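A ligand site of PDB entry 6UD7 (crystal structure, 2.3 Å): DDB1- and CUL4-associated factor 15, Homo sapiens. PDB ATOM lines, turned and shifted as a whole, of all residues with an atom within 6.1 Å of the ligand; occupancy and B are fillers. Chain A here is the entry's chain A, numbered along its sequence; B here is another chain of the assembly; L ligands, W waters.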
ATOM      1  N   THR A 231      22.034  19.473  -4.481  1.00  0.00           N
ATOM      2  CA  THR A 231      22.847  19.191  -5.666  1.00  0.00           C
ATOM      3  C   THR A 231      22.101  19.612  -6.915  1.00  0.00           C
ATOM      4  O   THR A 231      20.863  19.602  -6.931  1.00  0.00           O
ATOM      5  CB  THR A 231      23.188  17.693  -5.721  1.00  0.00           C
ATOM      6  OG1 THR A 231      21.986  16.937  -5.646  1.00  0.00           O
ATOM      7  CG2 THR A 231      24.153  17.256  -4.617  1.00  0.00           C
ATOM      8  N   PHE A 232      22.870  19.985  -7.945  1.00  0.00           N
ATOM      9  CA  PHE A 232      22.328  20.382  -9.248  1.00  0.00           C
ATOM     10  C   PHE A 232      22.347  19.139 -10.138  1.00  0.00           C
ATOM     11  O   PHE A 232      23.431  18.619 -10.443  1.00  0.00           O
ATOM     12  CB  PHE A 232      23.144  21.539  -9.849  1.00  0.00           C
ATOM     13  CG  PHE A 232      23.157  22.783  -8.983  1.00  0.00           C
ATOM     14  CD1 PHE A 232      22.159  23.746  -9.118  1.00  0.00           C
ATOM     15  CD2 PHE A 232      24.152  22.981  -8.033  1.00  0.00           C
ATOM     16  CE1 PHE A 232      22.165  24.892  -8.317  1.00  0.00           C
ATOM     17  CE2 PHE A 232      24.150  24.120  -7.224  1.00  0.00           C
ATOM     18  CZ  PHE A 232      23.153  25.069  -7.368  1.00  0.00           C
ATOM     19  N   GLN A 233      21.168  18.632 -10.518  1.00  0.00           N
ATOM     20  CA  GLN A 233      21.024  17.429 -11.338  1.00  0.00           C
ATOM     21  C   GLN A 233      20.162  17.683 -12.585  1.00  0.00           C
ATOM     22  O   GLN A 233      19.063  17.110 -12.703  1.00  0.00           O
ATOM     23  CB  GLN A 233      20.415  16.305 -10.489  1.00  0.00           C
ATOM     24  CG  GLN A 233      21.140  16.051  -9.191  1.00  0.00           C
ATOM     25  CD  GLN A 233      20.410  15.001  -8.407  1.00  0.00           C
ATOM     26  OE1 GLN A 233      19.544  15.318  -7.597  1.00  0.00           O
ATOM     27  NE2 GLN A 233      20.752  13.743  -8.651  1.00  0.00           N
ATOM     28  N   PRO A 234      20.661  18.476 -13.560  1.00  0.00           N
ATOM     29  CA  PRO A 234      19.833  18.820 -14.734  1.00  0.00           C
ATOM     30  C   PRO A 234      19.342  17.653 -15.593  1.00  0.00           C
ATOM     31  O   PRO A 234      18.250  17.786 -16.171  1.00  0.00           O
ATOM     32  CB  PRO A 234      20.734  19.774 -15.535  1.00  0.00           C
ATOM     33  CG  PRO A 234      22.088  19.532 -15.037  1.00  0.00           C
ATOM     34  CD  PRO A 234      21.938  19.208 -13.605  1.00  0.00           C
ATOM     35  N   ALA A 235      20.113  16.545 -15.691  1.00  0.00           N
ATOM     36  CA  ALA A 235      19.684  15.387 -16.496  1.00  0.00           C
ATOM     37  C   ALA A 235      18.422  14.732 -15.918  1.00  0.00           C
ATOM     38  O   ALA A 235      17.541  14.340 -16.692  1.00  0.00           O
ATOM     39  CB  ALA A 235      20.796  14.373 -16.636  1.00  0.00           C
ATOM     40  N   PHE A 236      18.312  14.684 -14.574  1.00  0.00           N
ATOM     41  CA  PHE A 236      17.148  14.112 -13.879  1.00  0.00           C
ATOM     42  C   PHE A 236      16.023  15.128 -13.704  1.00  0.00           C
ATOM     43  O   PHE A 236      14.866  14.787 -13.950  1.00  0.00           O
ATOM     44  CB  PHE A 236      17.528  13.540 -12.510  1.00  0.00           C
ATOM     45  CG  PHE A 236      18.287  12.247 -12.535  1.00  0.00           C
ATOM     46  CD1 PHE A 236      18.005  11.265 -13.485  1.00  0.00           C
ATOM     47  CD2 PHE A 236      19.265  11.975 -11.589  1.00  0.00           C
ATOM     48  CE1 PHE A 236      18.718  10.064 -13.521  1.00  0.00           C
ATOM     49  CE2 PHE A 236      19.976  10.779 -11.612  1.00  0.00           C
ATOM     50  CZ  PHE A 236      19.711   9.840 -12.590  1.00  0.00           C
ATOM     51  N   GLN A 237      16.364  16.379 -13.294  1.00  0.00           N
ATOM     52  CA  GLN A 237      15.415  17.483 -13.073  1.00  0.00           C
ATOM     53  C   GLN A 237      14.561  17.790 -14.293  1.00  0.00           C
ATOM     54  O   GLN A 237      13.455  18.303 -14.150  1.00  0.00           O
ATOM     55  CB  GLN A 237      16.143  18.760 -12.625  1.00  0.00           C
ATOM     56  CG  GLN A 237      16.704  18.712 -11.212  1.00  0.00           C
ATOM     57  CD  GLN A 237      17.476  19.972 -10.895  1.00  0.00           C
ATOM     58  OE1 GLN A 237      18.706  20.009 -10.921  1.00  0.00           O
ATOM     59  NE2 GLN A 237      16.763  21.038 -10.617  1.00  0.00           N
ATOM     60  N   VAL A 478      18.582  13.684  -2.959  1.00  0.00           N
ATOM     61  CA  VAL A 478      19.238  13.484  -4.249  1.00  0.00           C
ATOM     62  C   VAL A 478      18.312  12.615  -5.107  1.00  0.00           C
ATOM     63  O   VAL A 478      17.825  11.600  -4.621  1.00  0.00           O
ATOM     64  CB  VAL A 478      20.641  12.826  -4.070  1.00  0.00           C
ATOM     65  CG1 VAL A 478      21.315  12.534  -5.406  1.00  0.00           C
ATOM     66  CG2 VAL A 478      21.564  13.672  -3.189  1.00  0.00           C
ATOM     67  N   ILE A 479      18.059  13.007  -6.377  1.00  0.00           N
ATOM     68  CA  ILE A 479      17.233  12.228  -7.303  1.00  0.00           C
ATOM     69  C   ILE A 479      18.080  11.054  -7.838  1.00  0.00           C
ATOM     70  O   ILE A 479      19.236  11.267  -8.233  1.00  0.00           O
ATOM     71  CB  ILE A 479      16.616  13.102  -8.444  1.00  0.00           C
ATOM     72  CG1 ILE A 479      15.667  14.183  -7.878  1.00  0.00           C
ATOM     73  CG2 ILE A 479      15.893  12.256  -9.487  1.00  0.00           C
ATOM     74  CD1 ILE A 479      15.431  15.423  -8.810  1.00  0.00           C
ATOM     75  N   ARG A 553      26.657  11.554  -0.721  1.00  0.00           N
ATOM     76  CA  ARG A 553      26.568  11.960  -2.120  1.00  0.00           C
ATOM     77  C   ARG A 553      27.462  11.112  -3.011  1.00  0.00           C
ATOM     78  O   ARG A 553      27.075  10.843  -4.145  1.00  0.00           O
ATOM     79  CB  ARG A 553      26.828  13.455  -2.267  1.00  0.00           C
ATOM     80  CG  ARG A 553      25.642  14.287  -1.813  1.00  0.00           C
ATOM     81  CD  ARG A 553      26.068  15.708  -1.604  1.00  0.00           C
ATOM     82  NE  ARG A 553      24.945  16.562  -1.231  1.00  0.00           N
ATOM     83  CZ  ARG A 553      24.963  17.890  -1.268  1.00  0.00           C
ATOM     84  NH1 ARG A 553      26.039  18.533  -1.715  1.00  0.00           N
ATOM     85  NH2 ARG A 553      23.891  18.590  -0.905  1.00  0.00           N
ATOM     86  N   LYS A 554      28.606  10.608  -2.485  1.00  0.00           N
ATOM     87  CA  LYS A 554      29.458   9.656  -3.230  1.00  0.00           C
ATOM     88  C   LYS A 554      28.670   8.349  -3.441  1.00  0.00           C
ATOM     89  O   LYS A 554      28.766   7.753  -4.511  1.00  0.00           O
ATOM     90  CB  LYS A 554      30.754   9.355  -2.461  1.00  0.00           C
ATOM     91  CG  LYS A 554      31.934  10.263  -2.818  1.00  0.00           C
ATOM     92  CD  LYS A 554      32.971  10.288  -1.697  1.00  0.00           C
ATOM     93  CE  LYS A 554      33.978   9.162  -1.745  1.00  0.00           C
ATOM     94  NZ  LYS A 554      34.712   9.054  -0.454  1.00  0.00           N
ATOM     95  N   CYS A 556      25.383   8.058  -3.798  1.00  0.00           N
ATOM     96  CA  CYS A 556      24.355   8.383  -4.803  1.00  0.00           C
ATOM     97  C   CYS A 556      24.972   8.348  -6.199  1.00  0.00           C
ATOM     98  O   CYS A 556      24.352   7.821  -7.120  1.00  0.00           O
ATOM     99  CB  CYS A 556      23.723   9.738  -4.518  1.00  0.00           C
ATOM    100  SG  CYS A 556      22.779   9.811  -2.981  1.00  0.00           S
ATOM    101  N   VAL A 557      26.191   8.930  -6.368  1.00  0.00           N
ATOM    102  CA  VAL A 557      26.934   8.941  -7.629  1.00  0.00           C
ATOM    103  C   VAL A 557      27.237   7.484  -7.982  1.00  0.00           C
ATOM    104  O   VAL A 557      26.963   7.056  -9.105  1.00  0.00           O
ATOM    105  CB  VAL A 557      28.220   9.812  -7.586  1.00  0.00           C
ATOM    106  CG1 VAL A 557      29.044   9.665  -8.865  1.00  0.00           C
ATOM    107  CG2 VAL A 557      27.881  11.269  -7.323  1.00  0.00           C
ATOM    108  N   VAL A 560      23.873   5.732  -9.157  1.00  0.00           N
ATOM    109  CA  VAL A 560      23.508   6.237 -10.475  1.00  0.00           C
ATOM    110  C   VAL A 560      24.460   5.679 -11.563  1.00  0.00           C
ATOM    111  O   VAL A 560      23.975   5.182 -12.569  1.00  0.00           O
ATOM    112  CB  VAL A 560      23.406   7.790 -10.488  1.00  0.00           C
ATOM    113  CG1 VAL A 560      23.408   8.357 -11.907  1.00  0.00           C
ATOM    114  CG2 VAL A 560      22.180   8.263  -9.709  1.00  0.00           C
ATOM    115  N   MET A 561      25.790   5.724 -11.328  1.00  0.00           N
ATOM    116  CA  MET A 561      26.794   5.187 -12.269  1.00  0.00           C
ATOM    117  C   MET A 561      26.633   3.681 -12.490  1.00  0.00           C
ATOM    118  O   MET A 561      26.804   3.205 -13.606  1.00  0.00           O
ATOM    119  CB  MET A 561      28.238   5.469 -11.788  1.00  0.00           C
ATOM    120  CG  MET A 561      28.647   6.940 -11.791  1.00  0.00           C
ATOM    121  SD  MET A 561      28.398   7.775 -13.363  1.00  0.00           S
ATOM    122  CE  MET A 561      28.981   9.343 -12.973  1.00  0.00           C
ATOM    123  N   LEU A 564      23.568   2.731 -14.689  1.00  0.00           N
ATOM    124  CA  LEU A 564      23.589   3.490 -15.930  1.00  0.00           C
ATOM    125  C   LEU A 564      23.316   2.624 -17.174  1.00  0.00           C
ATOM    126  O   LEU A 564      23.962   1.599 -17.403  1.00  0.00           O
ATOM    127  CB  LEU A 564      24.911   4.263 -16.036  1.00  0.00           C
ATOM    128  CG  LEU A 564      25.134   5.235 -17.205  1.00  0.00           C
ATOM    129  CD1 LEU A 564      23.892   6.053 -17.521  1.00  0.00           C
ATOM    130  CD2 LEU A 564      26.277   6.160 -16.879  1.00  0.00           C
ATOM    131  N   ARG A 575      22.571  20.444 -21.905  1.00  0.00           N
ATOM    132  CA  ARG A 575      23.010  21.325 -20.843  1.00  0.00           C
ATOM    133  C   ARG A 575      24.147  22.205 -21.366  1.00  0.00           C
ATOM    134  O   ARG A 575      25.202  21.687 -21.754  1.00  0.00           O
ATOM    135  CB  ARG A 575      23.459  20.455 -19.642  1.00  0.00           C
ATOM    136  CG  ARG A 575      23.627  21.214 -18.347  1.00  0.00           C
ATOM    137  CD  ARG A 575      24.536  20.477 -17.395  1.00  0.00           C
ATOM    138  NE  ARG A 575      25.946  20.679 -17.717  1.00  0.00           N
ATOM    139  CZ  ARG A 575      26.724  21.597 -17.142  1.00  0.00           C
ATOM    140  NH1 ARG A 575      26.227  22.399 -16.206  1.00  0.00           N
ATOM    141  NH2 ARG A 575      27.992  21.706 -17.493  1.00  0.00           N
ATOM    142  N   ASN B  13      32.482   9.920 -16.678  1.00  0.00           N
ATOM    143  CA  ASN B  13      31.077  10.311 -16.568  1.00  0.00           C
ATOM    144  C   ASN B  13      30.791  11.280 -15.395  1.00  0.00           C
ATOM    145  O   ASN B  13      29.688  11.843 -15.324  1.00  0.00           O
ATOM    146  CB  ASN B  13      30.157   9.099 -16.531  1.00  0.00           C
ATOM    147  CG  ASN B  13      30.013   8.423 -17.861  1.00  0.00           C
ATOM    148  OD1 ASN B  13      30.598   8.838 -18.872  1.00  0.00           O
ATOM    149  ND2 ASN B  13      29.241   7.366 -17.885  1.00  0.00           N
ATOM    150  N   THR B  15      30.517  14.530 -13.551  1.00  0.00           N
ATOM    151  CA  THR B  15      30.287  15.921 -13.956  1.00  0.00           C
ATOM    152  C   THR B  15      30.800  16.902 -12.933  1.00  0.00           C
ATOM    153  O   THR B  15      31.038  16.529 -11.787  1.00  0.00           O
ATOM    154  CB  THR B  15      28.788  16.157 -14.188  1.00  0.00           C
ATOM    155  OG1 THR B  15      28.106  16.058 -12.930  1.00  0.00           O
ATOM    156  CG2 THR B  15      28.173  15.219 -15.215  1.00  0.00           C
ATOM    157  N   ASP B  17      29.041  19.311 -11.615  1.00  0.00           N
ATOM    158  CA  ASP B  17      27.965  19.382 -10.614  1.00  0.00           C
ATOM    159  C   ASP B  17      28.114  18.301  -9.544  1.00  0.00           C
ATOM    160  O   ASP B  17      27.856  18.587  -8.373  1.00  0.00           O
ATOM    161  CB  ASP B  17      26.584  19.252 -11.286  1.00  0.00           C
ATOM    162  CG  ASP B  17      26.351  20.256 -12.397  1.00  0.00           C
ATOM    163  OD1 ASP B  17      26.736  21.447 -12.233  1.00  0.00           O
ATOM    164  OD2 ASP B  17      25.760  19.866 -13.440  1.00  0.00           O
ATOM    165  N   MET B  18      28.560  17.070  -9.939  1.00  0.00           N
ATOM    166  CA  MET B  18      28.808  15.953  -9.020  1.00  0.00           C
ATOM    167  C   MET B  18      29.965  16.319  -8.095  1.00  0.00           C
ATOM    168  O   MET B  18      29.817  16.190  -6.888  1.00  0.00           O
ATOM    169  CB  MET B  18      29.086  14.648  -9.771  1.00  0.00           C
ATOM    170  CG  MET B  18      27.858  14.009 -10.341  1.00  0.00           C
ATOM    171  SD  MET B  18      28.226  12.710 -11.536  1.00  0.00           S
ATOM    172  CE  MET B  18      26.603  12.235 -11.971  1.00  0.00           C
ATOM    173  N   LEU B  19      31.074  16.860  -8.674  1.00  0.00           N
ATOM    174  CA  LEU B  19      32.256  17.324  -7.918  1.00  0.00           C
ATOM    175  C   LEU B  19      31.882  18.428  -6.934  1.00  0.00           C
ATOM    176  O   LEU B  19      32.405  18.449  -5.828  1.00  0.00           O
ATOM    177  CB  LEU B  19      33.347  17.832  -8.847  1.00  0.00           C
ATOM    178  CG  LEU B  19      34.127  16.770  -9.604  1.00  0.00           C
ATOM    179  CD1 LEU B  19      34.768  17.354 -10.820  1.00  0.00           C
ATOM    180  CD2 LEU B  19      35.179  16.135  -8.717  1.00  0.00           C
ATOM    181  N   GLY B  21      28.777  18.820  -5.590  1.00  0.00           N
ATOM    182  CA  GLY B  21      27.981  18.130  -4.584  1.00  0.00           C
ATOM    183  C   GLY B  21      28.810  17.354  -3.571  1.00  0.00           C
ATOM    184  O   GLY B  21      28.456  17.313  -2.396  1.00  0.00           O
ATOM    185  N   ILE B  22      29.926  16.774  -4.009  1.00  0.00           N
ATOM    186  CA  ILE B  22      30.828  15.974  -3.172  1.00  0.00           C
ATOM    187  C   ILE B  22      31.809  16.843  -2.342  1.00  0.00           C
ATOM    188  O   ILE B  22      32.195  16.424  -1.252  1.00  0.00           O
ATOM    189  CB  ILE B  22      31.538  14.924  -4.076  1.00  0.00           C
ATOM    190  CG1 ILE B  22      30.549  13.860  -4.597  1.00  0.00           C
ATOM    191  CG2 ILE B  22      32.756  14.263  -3.393  1.00  0.00           C
ATOM    192  CD1 ILE B  22      30.941  13.216  -5.924  1.00  0.00           C
HETATM  193  N1  LIG L   1      23.338  14.960 -11.973  1.00  0.00           N
HETATM  194  C1  LIG L   1      23.528  14.060 -10.931  1.00  0.00           C
HETATM  195  O1  LIG L   1      22.647  15.799 -14.201  1.00  0.00           O
HETATM  196  C2  LIG L   1      24.248  14.682  -9.859  1.00  0.00           C
HETATM  197  C3  LIG L   1      25.127  12.376 -15.339  1.00  0.00           C
HETATM  198  C4  LIG L   1      24.475  11.149 -15.356  1.00  0.00           C
HETATM  199  C5  LIG L   1      23.221  11.003 -14.782  1.00  0.00           C
HETATM  200  C6  LIG L   1      22.617  12.081 -14.175  1.00  0.00           C
HETATM  201  C7  LIG L   1      24.530  13.969  -8.678  1.00  0.00           C
HETATM  202  C8  LIG L   1      25.219  14.877  -7.787  1.00  0.00           C
HETATM  203  C9  LIG L   1      25.302  16.071  -8.474  1.00  0.00           C
HETATM  204  C10 LIG L   1      24.116  12.639  -8.552  1.00  0.00           C
HETATM  205  C11 LIG L   1      23.424  12.031  -9.585  1.00  0.00           C
HETATM  206  C12 LIG L   1      23.128  12.715 -10.758  1.00  0.00           C
HETATM  207  C13 LIG L   1      23.266  13.304 -14.142  1.00  0.00           C
HETATM  208  C14 LIG L   1      24.515  13.465 -14.730  1.00  0.00           C
HETATM  209  N2  LIG L   1      24.735  15.957  -9.722  1.00  0.00           N
HETATM  210  N3  LIG L   1      26.348  10.277 -17.153  1.00  0.00           N
HETATM  211  O2  LIG L   1      24.253   9.047 -16.829  1.00  0.00           O
HETATM  212  O3  LIG L   1      25.965   9.059 -15.065  1.00  0.00           O
HETATM  213  O4  LIG L   1      21.179  14.280 -12.973  1.00  0.00           O
HETATM  214  S1  LIG L   1      22.520  14.680 -13.312  1.00  0.00           S
HETATM  215  S2  LIG L   1      25.258   9.759 -16.105  1.00  0.00           S
HETATM  216 CL1  LIG L   1      25.796  14.431  -6.207  1.00  0.00          CL
HETATM  217  O   HOH W   1      28.119  12.518 -17.499  1.00  0.00           O
HETATM  218  O   HOH W   2      25.503  16.566 -13.273  1.00  0.00           O
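NE2 of Gln 233 lies within hydrogen-bond range of O of Ile 479 (2.9 Å).
The backbone NH (N) of Gln 233 sits at hydrogen-bond distance from the side-chain amide oxygen (OE1) of Gln 237, 2.8 Å away.
The backbone NH of Met 18 of chain B sits at hydrogen-bond distance from the side-chain hydroxyl of Thr 15 of chain B, at 3.2 Å.
OD2 of Asp 17 of chain B lies within salt-bridge range of NH1 of Arg 575, at 3.8 Å.
Water W1 bridges O of Asn 13 of chain B (2.8 Å) and N3 of the ligand (2.9 Å).
Water W2 lies within hydrogen-bond range of OG1 of Thr 15 of chain B (2.7 Å), N1 of the ligand (3.0 Å) and OD2 of Asp 17 of chain B (3.3 Å).
N of Pro 234 lies close to O1 of the ligand, 3.4 Å away.
The side-chain sulfur (SD) of Met 561 lies close to an oxygen (O3) of the ligand (3.2 Å).
Thr 231 touches the ligand.
Gln 233 touches the ligand.
Val 557 touches the ligand.
CG1 of Val 560 touches C5 of the ligand, at 3.9 Å.
CD1 of Leu 564 touches O2 of the ligand, at 3.1 Å.
O of Asp 17 of chain B touches C9 of the ligand (3.6 Å).
Met 18 of chain B touches the ligand.
Hydrophobic or aromatic side chains within 4 Å of the ligand: Pro 234, Ala 235, Phe 236, Val 557, Val 560, Met 561, Leu 564 and Met 18 of chain B.
12 residues have an atom within 4 Å of the ligand: Thr 231, Phe 232, Gln 233, Pro 234, Ala 235, Phe 236, Val 557, Val 560, Met 561, Leu 564, Asp 17 of chain B and Met 18 of chain B.
Along chain A the residues within 4 Å of the ligand span positions 231 to 564.
An oxygen (O1) of the ligand sits at hydrogen-bond distance from the backbone NH (N) of Ala 235, 3.0 Å away.
O of Phe 232 is in hydrogen-bond range of N2 of the ligand (3.1 Å).
An oxygen (O4) of the ligand sits close to the backbone NH of Phe 236, 3.3 Å away.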
